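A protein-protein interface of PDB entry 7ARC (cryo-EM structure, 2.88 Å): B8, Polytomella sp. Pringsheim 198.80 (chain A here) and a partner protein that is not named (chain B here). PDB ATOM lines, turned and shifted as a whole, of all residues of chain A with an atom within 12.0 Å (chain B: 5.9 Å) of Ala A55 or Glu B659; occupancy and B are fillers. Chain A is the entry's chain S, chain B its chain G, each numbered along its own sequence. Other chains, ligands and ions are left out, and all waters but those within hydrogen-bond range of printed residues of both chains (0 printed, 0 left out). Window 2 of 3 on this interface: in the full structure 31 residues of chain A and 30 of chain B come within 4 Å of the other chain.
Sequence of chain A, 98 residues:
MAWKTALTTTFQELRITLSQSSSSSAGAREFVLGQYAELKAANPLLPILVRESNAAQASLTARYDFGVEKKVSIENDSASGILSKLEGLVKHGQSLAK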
ATOM      1  N   ILE A  16      11.876  -6.387  15.223  1.00  0.00           N
ATOM      2  CA  ILE A  16      11.178  -7.021  16.338  1.00  0.00           C
ATOM      3  C   ILE A  16       9.896  -6.235  16.577  1.00  0.00           C
ATOM      4  O   ILE A  16       9.919  -5.171  17.205  1.00  0.00           O
ATOM      5  CB  ILE A  16      12.038  -7.077  17.604  1.00  0.00           C
ATOM      6  CG1 ILE A  16      13.279  -7.933  17.362  1.00  0.00           C
ATOM      7  CG2 ILE A  16      11.235  -7.645  18.759  1.00  0.00           C
ATOM      8  CD1 ILE A  16      14.306  -7.837  18.459  1.00  0.00           C
ATOM      9  N   THR A  17       8.775  -6.746  16.078  1.00  0.00           N
ATOM     10  CA  THR A  17       7.474  -6.136  16.312  1.00  0.00           C
ATOM     11  C   THR A  17       6.819  -6.753  17.543  1.00  0.00           C
ATOM     12  O   THR A  17       6.858  -7.971  17.733  1.00  0.00           O
ATOM     13  CB  THR A  17       6.570  -6.314  15.089  1.00  0.00           C
ATOM     14  OG1 THR A  17       7.040  -5.482  14.022  1.00  0.00           O
ATOM     15  CG2 THR A  17       5.132  -5.934  15.414  1.00  0.00           C
ATOM     16  N   LEU A  18       6.230  -5.908  18.385  1.00  0.00           N
ATOM     17  CA  LEU A  18       5.642  -6.381  19.632  1.00  0.00           C
ATOM     18  C   LEU A  18       4.558  -5.404  20.068  1.00  0.00           C
ATOM     19  O   LEU A  18       4.484  -4.276  19.579  1.00  0.00           O
ATOM     20  CB  LEU A  18       6.702  -6.558  20.726  1.00  0.00           C
ATOM     21  CG  LEU A  18       7.316  -5.324  21.387  1.00  0.00           C
ATOM     22  CD1 LEU A  18       8.032  -5.724  22.659  1.00  0.00           C
ATOM     23  CD2 LEU A  18       8.268  -4.612  20.452  1.00  0.00           C
ATOM     24  N   SER A  19       3.715  -5.855  20.991  1.00  0.00           N
ATOM     25  CA  SER A  19       2.672  -5.021  21.568  1.00  0.00           C
ATOM     26  C   SER A  19       3.146  -4.420  22.884  1.00  0.00           C
ATOM     27  O   SER A  19       3.807  -5.086  23.684  1.00  0.00           O
ATOM     28  CB  SER A  19       1.385  -5.812  21.793  1.00  0.00           C
ATOM     29  OG  SER A  19       0.572  -5.186  22.767  1.00  0.00           O
ATOM     30  N   GLN A  20       2.801  -3.148  23.094  1.00  0.00           N
ATOM     31  CA  GLN A  20       3.309  -2.410  24.245  1.00  0.00           C
ATOM     32  C   GLN A  20       2.834  -3.015  25.561  1.00  0.00           C
ATOM     33  O   GLN A  20       3.615  -3.142  26.511  1.00  0.00           O
ATOM     34  CB  GLN A  20       2.866  -0.954  24.143  1.00  0.00           C
ATOM     35  CG  GLN A  20       3.483  -0.227  22.976  1.00  0.00           C
ATOM     36  CD  GLN A  20       3.018   1.202  22.874  1.00  0.00           C
ATOM     37  OE1 GLN A  20       2.176   1.651  23.649  1.00  0.00           O
ATOM     38  NE2 GLN A  20       3.545   1.923  21.893  1.00  0.00           N
ATOM     39  N   SER A  21       1.558  -3.386  25.640  1.00  0.00           N
ATOM     40  CA  SER A  21       1.001  -4.024  26.835  1.00  0.00           C
ATOM     41  C   SER A  21       0.020  -5.103  26.387  1.00  0.00           C
ATOM     42  O   SER A  21      -1.116  -4.798  26.012  1.00  0.00           O
ATOM     43  CB  SER A  21       0.328  -3.002  27.742  1.00  0.00           C
ATOM     44  OG  SER A  21       1.268  -2.069  28.244  1.00  0.00           O
ATOM     45  N   SER A  22       0.460  -6.357  26.424  1.00  0.00           N
ATOM     46  CA  SER A  22      -0.399  -7.477  26.070  1.00  0.00           C
ATOM     47  C   SER A  22       0.152  -8.741  26.708  1.00  0.00           C
ATOM     48  O   SER A  22       1.343  -8.836  27.014  1.00  0.00           O
ATOM     49  CB  SER A  22      -0.512  -7.649  24.552  1.00  0.00           C
ATOM     50  OG  SER A  22      -1.140  -6.529  23.955  1.00  0.00           O
ATOM     51  N   SER A  23      -0.739  -9.713  26.913  1.00  0.00           N
ATOM     52  CA  SER A  23      -0.313 -10.994  27.463  1.00  0.00           C
ATOM     53  C   SER A  23       0.431 -11.823  26.428  1.00  0.00           C
ATOM     54  O   SER A  23       1.344 -12.578  26.780  1.00  0.00           O
ATOM     55  CB  SER A  23      -1.520 -11.766  27.994  1.00  0.00           C
ATOM     56  OG  SER A  23      -2.130 -11.086  29.078  1.00  0.00           O
ATOM     57  N   SER A  24       0.053 -11.703  25.153  1.00  0.00           N
ATOM     58  CA  SER A  24       0.744 -12.441  24.100  1.00  0.00           C
ATOM     59  C   SER A  24       2.173 -11.951  23.914  1.00  0.00           C
ATOM     60  O   SER A  24       3.064 -12.748  23.601  1.00  0.00           O
ATOM     61  CB  SER A  24      -0.032 -12.326  22.790  1.00  0.00           C
ATOM     62  OG  SER A  24      -1.305 -12.934  22.899  1.00  0.00           O
ATOM     63  N   SER A  25       2.409 -10.654  24.093  1.00  0.00           N
ATOM     64  CA  SER A  25       3.704 -10.047  23.826  1.00  0.00           C
ATOM     65  C   SER A  25       4.581  -9.947  25.067  1.00  0.00           C
ATOM     66  O   SER A  25       5.637  -9.312  25.012  1.00  0.00           O
ATOM     67  CB  SER A  25       3.516  -8.663  23.206  1.00  0.00           C
ATOM     68  OG  SER A  25       2.517  -8.703  22.202  1.00  0.00           O
ATOM     69  N   ALA A  26       4.159 -10.543  26.186  1.00  0.00           N
ATOM     70  CA  ALA A  26       4.973 -10.506  27.396  1.00  0.00           C
ATOM     71  C   ALA A  26       6.335 -11.150  27.165  1.00  0.00           C
ATOM     72  O   ALA A  26       7.364 -10.622  27.605  1.00  0.00           O
ATOM     73  CB  ALA A  26       4.239 -11.198  28.543  1.00  0.00           C
ATOM     74  N   ALA A  28       7.900 -11.458  24.277  1.00  0.00           N
ATOM     75  CA  ALA A  28       8.660 -10.568  23.405  1.00  0.00           C
ATOM     76  C   ALA A  28       9.226  -9.385  24.178  1.00  0.00           C
ATOM     77  O   ALA A  28      10.365  -8.965  23.940  1.00  0.00           O
ATOM     78  CB  ALA A  28       7.783 -10.085  22.252  1.00  0.00           C
ATOM     79  N   ARG A  29       8.441  -8.825  25.100  1.00  0.00           N
ATOM     80  CA  ARG A  29       8.935  -7.726  25.923  1.00  0.00           C
ATOM     81  C   ARG A  29      10.090  -8.174  26.810  1.00  0.00           C
ATOM     82  O   ARG A  29      11.089  -7.460  26.949  1.00  0.00           O
ATOM     83  CB  ARG A  29       7.792  -7.139  26.751  1.00  0.00           C
ATOM     84  CG  ARG A  29       7.348  -5.769  26.265  1.00  0.00           C
ATOM     85  CD  ARG A  29       6.190  -5.195  27.064  1.00  0.00           C
ATOM     86  NE  ARG A  29       4.950  -5.936  26.869  1.00  0.00           N
ATOM     87  CZ  ARG A  29       4.444  -6.802  27.735  1.00  0.00           C
ATOM     88  NH1 ARG A  29       5.049  -7.066  28.881  1.00  0.00           N
ATOM     89  NH2 ARG A  29       3.299  -7.412  27.448  1.00  0.00           N
ATOM     90  N   ARG A  51       9.900  -2.141  17.133  1.00  0.00           N
ATOM     91  CA  ARG A  51       8.748  -1.312  16.816  1.00  0.00           C
ATOM     92  C   ARG A  51       7.528  -1.853  17.546  1.00  0.00           C
ATOM     93  O   ARG A  51       7.303  -3.064  17.577  1.00  0.00           O
ATOM     94  CB  ARG A  51       8.490  -1.284  15.308  1.00  0.00           C
ATOM     95  CG  ARG A  51       9.603  -0.636  14.504  1.00  0.00           C
ATOM     96  CD  ARG A  51       9.741   0.841  14.803  1.00  0.00           C
ATOM     97  NE  ARG A  51      10.828   1.436  14.036  1.00  0.00           N
ATOM     98  CZ  ARG A  51      12.063   1.594  14.488  1.00  0.00           C
ATOM     99  NH1 ARG A  51      12.409   1.211  15.703  1.00  0.00           N
ATOM    100  NH2 ARG A  51      12.978   2.143  13.695  1.00  0.00           N
ATOM    101  N   GLU A  52       6.739  -0.954  18.126  1.00  0.00           N
ATOM    102  CA  GLU A  52       5.685  -1.355  19.043  1.00  0.00           C
ATOM    103  C   GLU A  52       4.417  -0.548  18.809  1.00  0.00           C
ATOM    104  O   GLU A  52       4.473   0.633  18.459  1.00  0.00           O
ATOM    105  CB  GLU A  52       6.164  -1.206  20.493  1.00  0.00           C
ATOM    106  CG  GLU A  52       6.365   0.230  20.944  1.00  0.00           C
ATOM    107  CD  GLU A  52       7.734   0.773  20.569  1.00  0.00           C
ATOM    108  OE1 GLU A  52       8.409   0.163  19.717  1.00  0.00           O
ATOM    109  OE2 GLU A  52       8.140   1.810  21.129  1.00  0.00           O
ATOM    110  N   SER A  53       3.276  -1.210  18.988  1.00  0.00           N
ATOM    111  CA  SER A  53       1.970  -0.568  18.980  1.00  0.00           C
ATOM    112  C   SER A  53       1.031  -1.373  19.866  1.00  0.00           C
ATOM    113  O   SER A  53       1.266  -2.553  20.131  1.00  0.00           O
ATOM    114  CB  SER A  53       1.405  -0.449  17.560  1.00  0.00           C
ATOM    115  OG  SER A  53       0.014  -0.181  17.587  1.00  0.00           O
ATOM    116  N   ASN A  54      -0.041  -0.721  20.328  1.00  0.00           N
ATOM    117  CA  ASN A  54      -0.941  -1.368  21.279  1.00  0.00           C
ATOM    118  C   ASN A  54      -1.615  -2.592  20.674  1.00  0.00           C
ATOM    119  O   ASN A  54      -1.709  -3.641  21.321  1.00  0.00           O
ATOM    120  CB  ASN A  54      -1.996  -0.377  21.770  1.00  0.00           C
ATOM    121  CG  ASN A  54      -1.420   0.696  22.667  1.00  0.00           C
ATOM    122  OD1 ASN A  54      -0.581   0.419  23.525  1.00  0.00           O
ATOM    123  ND2 ASN A  54      -1.869   1.931  22.478  1.00  0.00           N
ATOM    124  N   ALA A  55      -2.084  -2.484  19.435  1.00  0.00           N
ATOM    125  CA  ALA A  55      -2.736  -3.589  18.746  1.00  0.00           C
ATOM    126  C   ALA A  55      -1.771  -4.414  17.907  1.00  0.00           C
ATOM    127  O   ALA A  55      -2.211  -5.316  17.187  1.00  0.00           O
ATOM    128  CB  ALA A  55      -3.871  -3.065  17.865  1.00  0.00           C
ATOM    129  N   ALA A  56      -0.477  -4.120  17.975  1.00  0.00           N
ATOM    130  CA  ALA A  56       0.502  -4.831  17.170  1.00  0.00           C
ATOM    131  C   ALA A  56       0.573  -6.303  17.562  1.00  0.00           C
ATOM    132  O   ALA A  56       0.391  -6.672  18.724  1.00  0.00           O
ATOM    133  CB  ALA A  56       1.879  -4.188  17.324  1.00  0.00           C
ATOM    134  N   GLN A  57       0.840  -7.146  16.571  1.00  0.00           N
ATOM    135  CA  GLN A  57       0.963  -8.582  16.770  1.00  0.00           C
ATOM    136  C   GLN A  57       2.442  -8.942  16.742  1.00  0.00           C
ATOM    137  O   GLN A  57       3.158  -8.559  15.811  1.00  0.00           O
ATOM    138  CB  GLN A  57       0.204  -9.355  15.692  1.00  0.00           C
ATOM    139  CG  GLN A  57      -1.303  -9.129  15.689  1.00  0.00           C
ATOM    140  CD  GLN A  57      -1.987  -9.666  16.934  1.00  0.00           C
ATOM    141  OE1 GLN A  57      -2.913  -9.050  17.463  1.00  0.00           O
ATOM    142  NE2 GLN A  57      -1.541 -10.824  17.402  1.00  0.00           N
ATOM    143  N   ALA A  58       2.893  -9.668  17.762  1.00  0.00           N
ATOM    144  CA  ALA A  58       4.318  -9.917  17.932  1.00  0.00           C
ATOM    145  C   ALA A  58       4.871 -10.752  16.782  1.00  0.00           C
ATOM    146  O   ALA A  58       4.263 -11.739  16.360  1.00  0.00           O
ATOM    147  CB  ALA A  58       4.572 -10.616  19.266  1.00  0.00           C
ATOM    148  N   SER A  59       6.033 -10.347  16.275  1.00  0.00           N
ATOM    149  CA  SER A  59       6.672 -11.046  15.168  1.00  0.00           C
ATOM    150  C   SER A  59       8.161 -10.740  15.185  1.00  0.00           C
ATOM    151  O   SER A  59       8.608  -9.767  15.796  1.00  0.00           O
ATOM    152  CB  SER A  59       6.057 -10.660  13.818  1.00  0.00           C
ATOM    153  OG  SER A  59       6.306  -9.300  13.510  1.00  0.00           O
ATOM    154  N   SER A  73       6.385 -15.605  13.567  1.00  0.00           N
ATOM    155  CA  SER A  73       5.537 -15.169  14.667  1.00  0.00           C
ATOM    156  C   SER A  73       6.142 -15.585  16.002  1.00  0.00           C
ATOM    157  O   SER A  73       6.606 -16.716  16.168  1.00  0.00           O
ATOM    158  CB  SER A  73       4.134 -15.752  14.524  1.00  0.00           C
ATOM    159  OG  SER A  73       3.467 -15.768  15.772  1.00  0.00           O
ATOM    160  N   GLU A  75       4.456 -14.915  19.087  1.00  0.00           N
ATOM    161  CA  GLU A  75       3.415 -14.708  20.084  1.00  0.00           C
ATOM    162  C   GLU A  75       3.400 -15.844  21.100  1.00  0.00           C
ATOM    163  O   GLU A  75       3.555 -17.015  20.748  1.00  0.00           O
ATOM    164  CB  GLU A  75       2.049 -14.585  19.413  1.00  0.00           C
ATOM    165  CG  GLU A  75       1.906 -13.344  18.560  1.00  0.00           C
ATOM    166  CD  GLU A  75       0.555 -13.255  17.888  1.00  0.00           C
ATOM    167  OE1 GLU A  75      -0.227 -14.223  17.995  1.00  0.00           O
ATOM    168  OE2 GLU A  75       0.275 -12.221  17.249  1.00  0.00           O
ATOM    169  N   VAL B 607       1.358   9.803  13.615  1.00  0.00           N
ATOM    170  CA  VAL B 607       1.239   9.638  12.171  1.00  0.00           C
ATOM    171  C   VAL B 607       0.054  10.465  11.687  1.00  0.00           C
ATOM    172  O   VAL B 607      -1.081  10.262  12.130  1.00  0.00           O
ATOM    173  CB  VAL B 607       1.082   8.161  11.787  1.00  0.00           C
ATOM    174  CG1 VAL B 607       0.945   8.023  10.285  1.00  0.00           C
ATOM    175  CG2 VAL B 607       2.273   7.368  12.284  1.00  0.00           C
ATOM    176  N   PRO B 655       4.112  -1.016  13.038  1.00  0.00           N
ATOM    177  CA  PRO B 655       2.675  -1.119  13.336  1.00  0.00           C
ATOM    178  C   PRO B 655       1.992   0.204  13.642  1.00  0.00           C
ATOM    179  O   PRO B 655       0.783   0.324  13.409  1.00  0.00           O
ATOM    180  CB  PRO B 655       2.643  -2.066  14.542  1.00  0.00           C
ATOM    181  CG  PRO B 655       3.988  -1.935  15.161  1.00  0.00           C
ATOM    182  CD  PRO B 655       4.934  -1.739  14.020  1.00  0.00           C
ATOM    183  N   HIS B 656       2.713   1.198  14.167  1.00  0.00           N
ATOM    184  CA  HIS B 656       2.060   2.449  14.543  1.00  0.00           C
ATOM    185  C   HIS B 656       1.510   3.190  13.331  1.00  0.00           C
ATOM    186  O   HIS B 656       0.564   3.973  13.465  1.00  0.00           O
ATOM    187  CB  HIS B 656       3.019   3.355  15.315  1.00  0.00           C
ATOM    188  CG  HIS B 656       4.348   3.535  14.655  1.00  0.00           C
ATOM    189  ND1 HIS B 656       4.737   4.730  14.088  1.00  0.00           N
ATOM    190  CD2 HIS B 656       5.393   2.688  14.503  1.00  0.00           C
ATOM    191  CE1 HIS B 656       5.951   4.600  13.585  1.00  0.00           C
ATOM    192  NE2 HIS B 656       6.375   3.374  13.832  1.00  0.00           N
ATOM    193  N   PHE B 657       2.093   2.974  12.150  1.00  0.00           N
ATOM    194  CA  PHE B 657       1.598   3.617  10.937  1.00  0.00           C
ATOM    195  C   PHE B 657       0.153   3.253  10.627  1.00  0.00           C
ATOM    196  O   PHE B 657      -0.518   4.000   9.910  1.00  0.00           O
ATOM    197  CB  PHE B 657       2.491   3.272   9.748  1.00  0.00           C
ATOM    198  CG  PHE B 657       3.655   4.201   9.583  1.00  0.00           C
ATOM    199  CD1 PHE B 657       3.484   5.448   9.009  1.00  0.00           C
ATOM    200  CD2 PHE B 657       4.918   3.833  10.006  1.00  0.00           C
ATOM    201  CE1 PHE B 657       4.548   6.309   8.859  1.00  0.00           C
ATOM    202  CE2 PHE B 657       5.987   4.691   9.858  1.00  0.00           C
ATOM    203  CZ  PHE B 657       5.801   5.931   9.283  1.00  0.00           C
ATOM    204  N   ALA B 658      -0.337   2.120  11.133  1.00  0.00           N
ATOM    205  CA  ALA B 658      -1.751   1.801  10.979  1.00  0.00           C
ATOM    206  C   ALA B 658      -2.625   2.718  11.826  1.00  0.00           C
ATOM    207  O   ALA B 658      -3.780   2.976  11.472  1.00  0.00           O
ATOM    208  CB  ALA B 658      -2.004   0.339  11.346  1.00  0.00           C
ATOM    209  N   GLU B 659      -2.100   3.193  12.955  1.00  0.00           N
ATOM    210  CA  GLU B 659      -2.835   4.067  13.868  1.00  0.00           C
ATOM    211  C   GLU B 659      -2.603   5.519  13.457  1.00  0.00           C
ATOM    212  O   GLU B 659      -1.846   6.264  14.082  1.00  0.00           O
ATOM    213  CB  GLU B 659      -2.406   3.809  15.306  1.00  0.00           C
ATOM    214  CG  GLU B 659      -2.266   2.332  15.667  1.00  0.00           C
ATOM    215  CD  GLU B 659      -3.592   1.650  15.969  1.00  0.00           C
ATOM    216  OE1 GLU B 659      -4.626   2.032  15.383  1.00  0.00           O
ATOM    217  OE2 GLU B 659      -3.597   0.717  16.800  1.00  0.00           O
ATOM    218  N   ILE B 660      -3.272   5.927  12.378  1.00  0.00           N
ATOM    219  CA  ILE B 660      -3.150   7.303  11.909  1.00  0.00           C
ATOM    220  C   ILE B 660      -3.867   8.230  12.880  1.00  0.00           C
ATOM    221  O   ILE B 660      -5.024   7.994  13.253  1.00  0.00           O
ATOM    222  CB  ILE B 660      -3.712   7.460  10.487  1.00  0.00           C
ATOM    223  CG1 ILE B 660      -2.931   6.624   9.470  1.00  0.00           C
ATOM    224  CG2 ILE B 660      -3.698   8.918  10.063  1.00  0.00           C
ATOM    225  CD1 ILE B 660      -3.444   5.220   9.288  1.00  0.00           C
ATOM    226  N   GLY B 661      -3.180   9.294  13.296  1.00  0.00           N
ATOM    227  CA  GLY B 661      -3.750  10.281  14.181  1.00  0.00           C
ATOM    228  C   GLY B 661      -3.521  10.036  15.655  1.00  0.00           C
ATOM    229  O   GLY B 661      -3.878  10.894  16.472  1.00  0.00           O
ATOM    230  N   LYS B 662      -2.943   8.898  16.026  1.00  0.00           N
ATOM    231  CA  LYS B 662      -2.707   8.544  17.417  1.00  0.00           C
ATOM    232  C   LYS B 662      -1.214   8.377  17.649  1.00  0.00           C
ATOM    233  O   LYS B 662      -0.532   7.708  16.866  1.00  0.00           O
ATOM    234  CB  LYS B 662      -3.443   7.256  17.792  1.00  0.00           C
ATOM    235  CG  LYS B 662      -4.955   7.353  17.716  1.00  0.00           C
ATOM    236  CD  LYS B 662      -5.606   6.059  18.167  1.00  0.00           C
ATOM    237  CE  LYS B 662      -5.382   4.943  17.159  1.00  0.00           C
ATOM    238  NZ  LYS B 662      -6.067   5.207  15.864  1.00  0.00           N
ATOM    239  N   ALA B 663      -0.709   8.988  18.717  1.00  0.00           N
ATOM    240  CA  ALA B 663       0.679   8.797  19.112  1.00  0.00           C
ATOM    241  C   ALA B 663       0.805   7.543  19.966  1.00  0.00           C
ATOM    242  O   ALA B 663       0.052   7.357  20.926  1.00  0.00           O
ATOM    243  CB  ALA B 663       1.193  10.016  19.877  1.00  0.00           C
ATOM    244  N   GLU B 664       1.756   6.684  19.615  1.00  0.00           N
ATOM    245  CA  GLU B 664       1.991   5.434  20.324  1.00  0.00           C
ATOM    246  C   GLU B 664       3.158   5.603  21.284  1.00  0.00           C
ATOM    247  O   GLU B 664       4.194   6.166  20.917  1.00  0.00           O
ATOM    248  CB  GLU B 664       2.280   4.297  19.344  1.00  0.00           C
ATOM    249  CG  GLU B 664       1.105   3.913  18.461  1.00  0.00           C
ATOM    250  CD  GLU B 664      -0.002   3.224  19.231  1.00  0.00           C
ATOM    251  OE1 GLU B 664       0.308   2.336  20.054  1.00  0.00           O
ATOM    252  OE2 GLU B 664      -1.182   3.565  19.009  1.00  0.00           O
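The backbone NH (N) of Asn A54 sits at hydrogen-bond distance from the side-chain carboxylate (OE1) of Glu B664, at 3.1 Å.
O of Ile A16 lies within hydrogen-bond range of N of Arg A51 (3.0 Å). O of Arg A51 sits at hydrogen-bond distance from N of Leu A18 (3.1 Å). OG of Ser A19 sits at hydrogen-bond distance from O of Asn A54. O of Ser A53 lies within hydrogen-bond range of N of Gln A20, at 3.4 Å. The side-chain amide oxygen of Asn A54 sits close to the side-chain amide oxygen of Gln A20 (3.0 Å). The side-chain carboxylate of Glu B659 lies within salt-bridge range of the side-chain amino group of Lys B662 (3.5 Å).
Among the printed residues, merely in contact across the chains: Ser A53 with Glu B664 (3.5 Å), Ala A56 with Pro B655 (3.6 Å), Ser A53 with Pro B655 (3.6 Å), Gln A20 with Glu B664 (3.7 Å), Ser A53 with Glu B659 (3.8 Å), Arg A51 with Pro B655 (3.8 Å), Glu A52 with Pro B655 (3.9 Å), Ala A55 with Glu B659 (3.9 Å) and Ser A53 with His B656 (3.99 Å).
Ser A24 touches none of the printed residues of chain B. Printed residues of chain B within 4 Å of Glu A52: Pro B655. Of chain B, only Glu B659 (3.9 Å) comes within 4 Å of Ala A55. No residue of chain A comes within 4 Å of Val B607. Glu B659 touches just these residues of chain A: Ser A53 and Ala A55. No residue of chain A comes within 4 Å of Ile B660. No residue of chain A comes within 4 Å of Gly B661. No residue of chain A comes within 4 Å of Lys B662. Of the printed residues of chain A, Glu B664 touches Gln A20 (3.7 Å), Ser A53 (3.5 Å) and Asn A54 (3.1 Å). The nearest residue of chain A that does not touch Glu B659 is Asn A54 (5.2 Å).
Of the 11 printed residues of chain B, 4 touch a printed residue of chain A. Printed residues of chain B that touch a printed residue of chain A: Pro B655, His B656, Glu B659 and Glu B664. Of the 24 printed residues of chain A, 7 touch a printed residue of chain B. Hydrophobic or aromatic side chains of chain A within 4 Å of the printed part of chain B: Ala A55 and Ala A56. Among the printed residues, no Asp or Glu carboxylate lies within 4 Å of a Lys or Arg side-chain nitrogen of the other chain.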
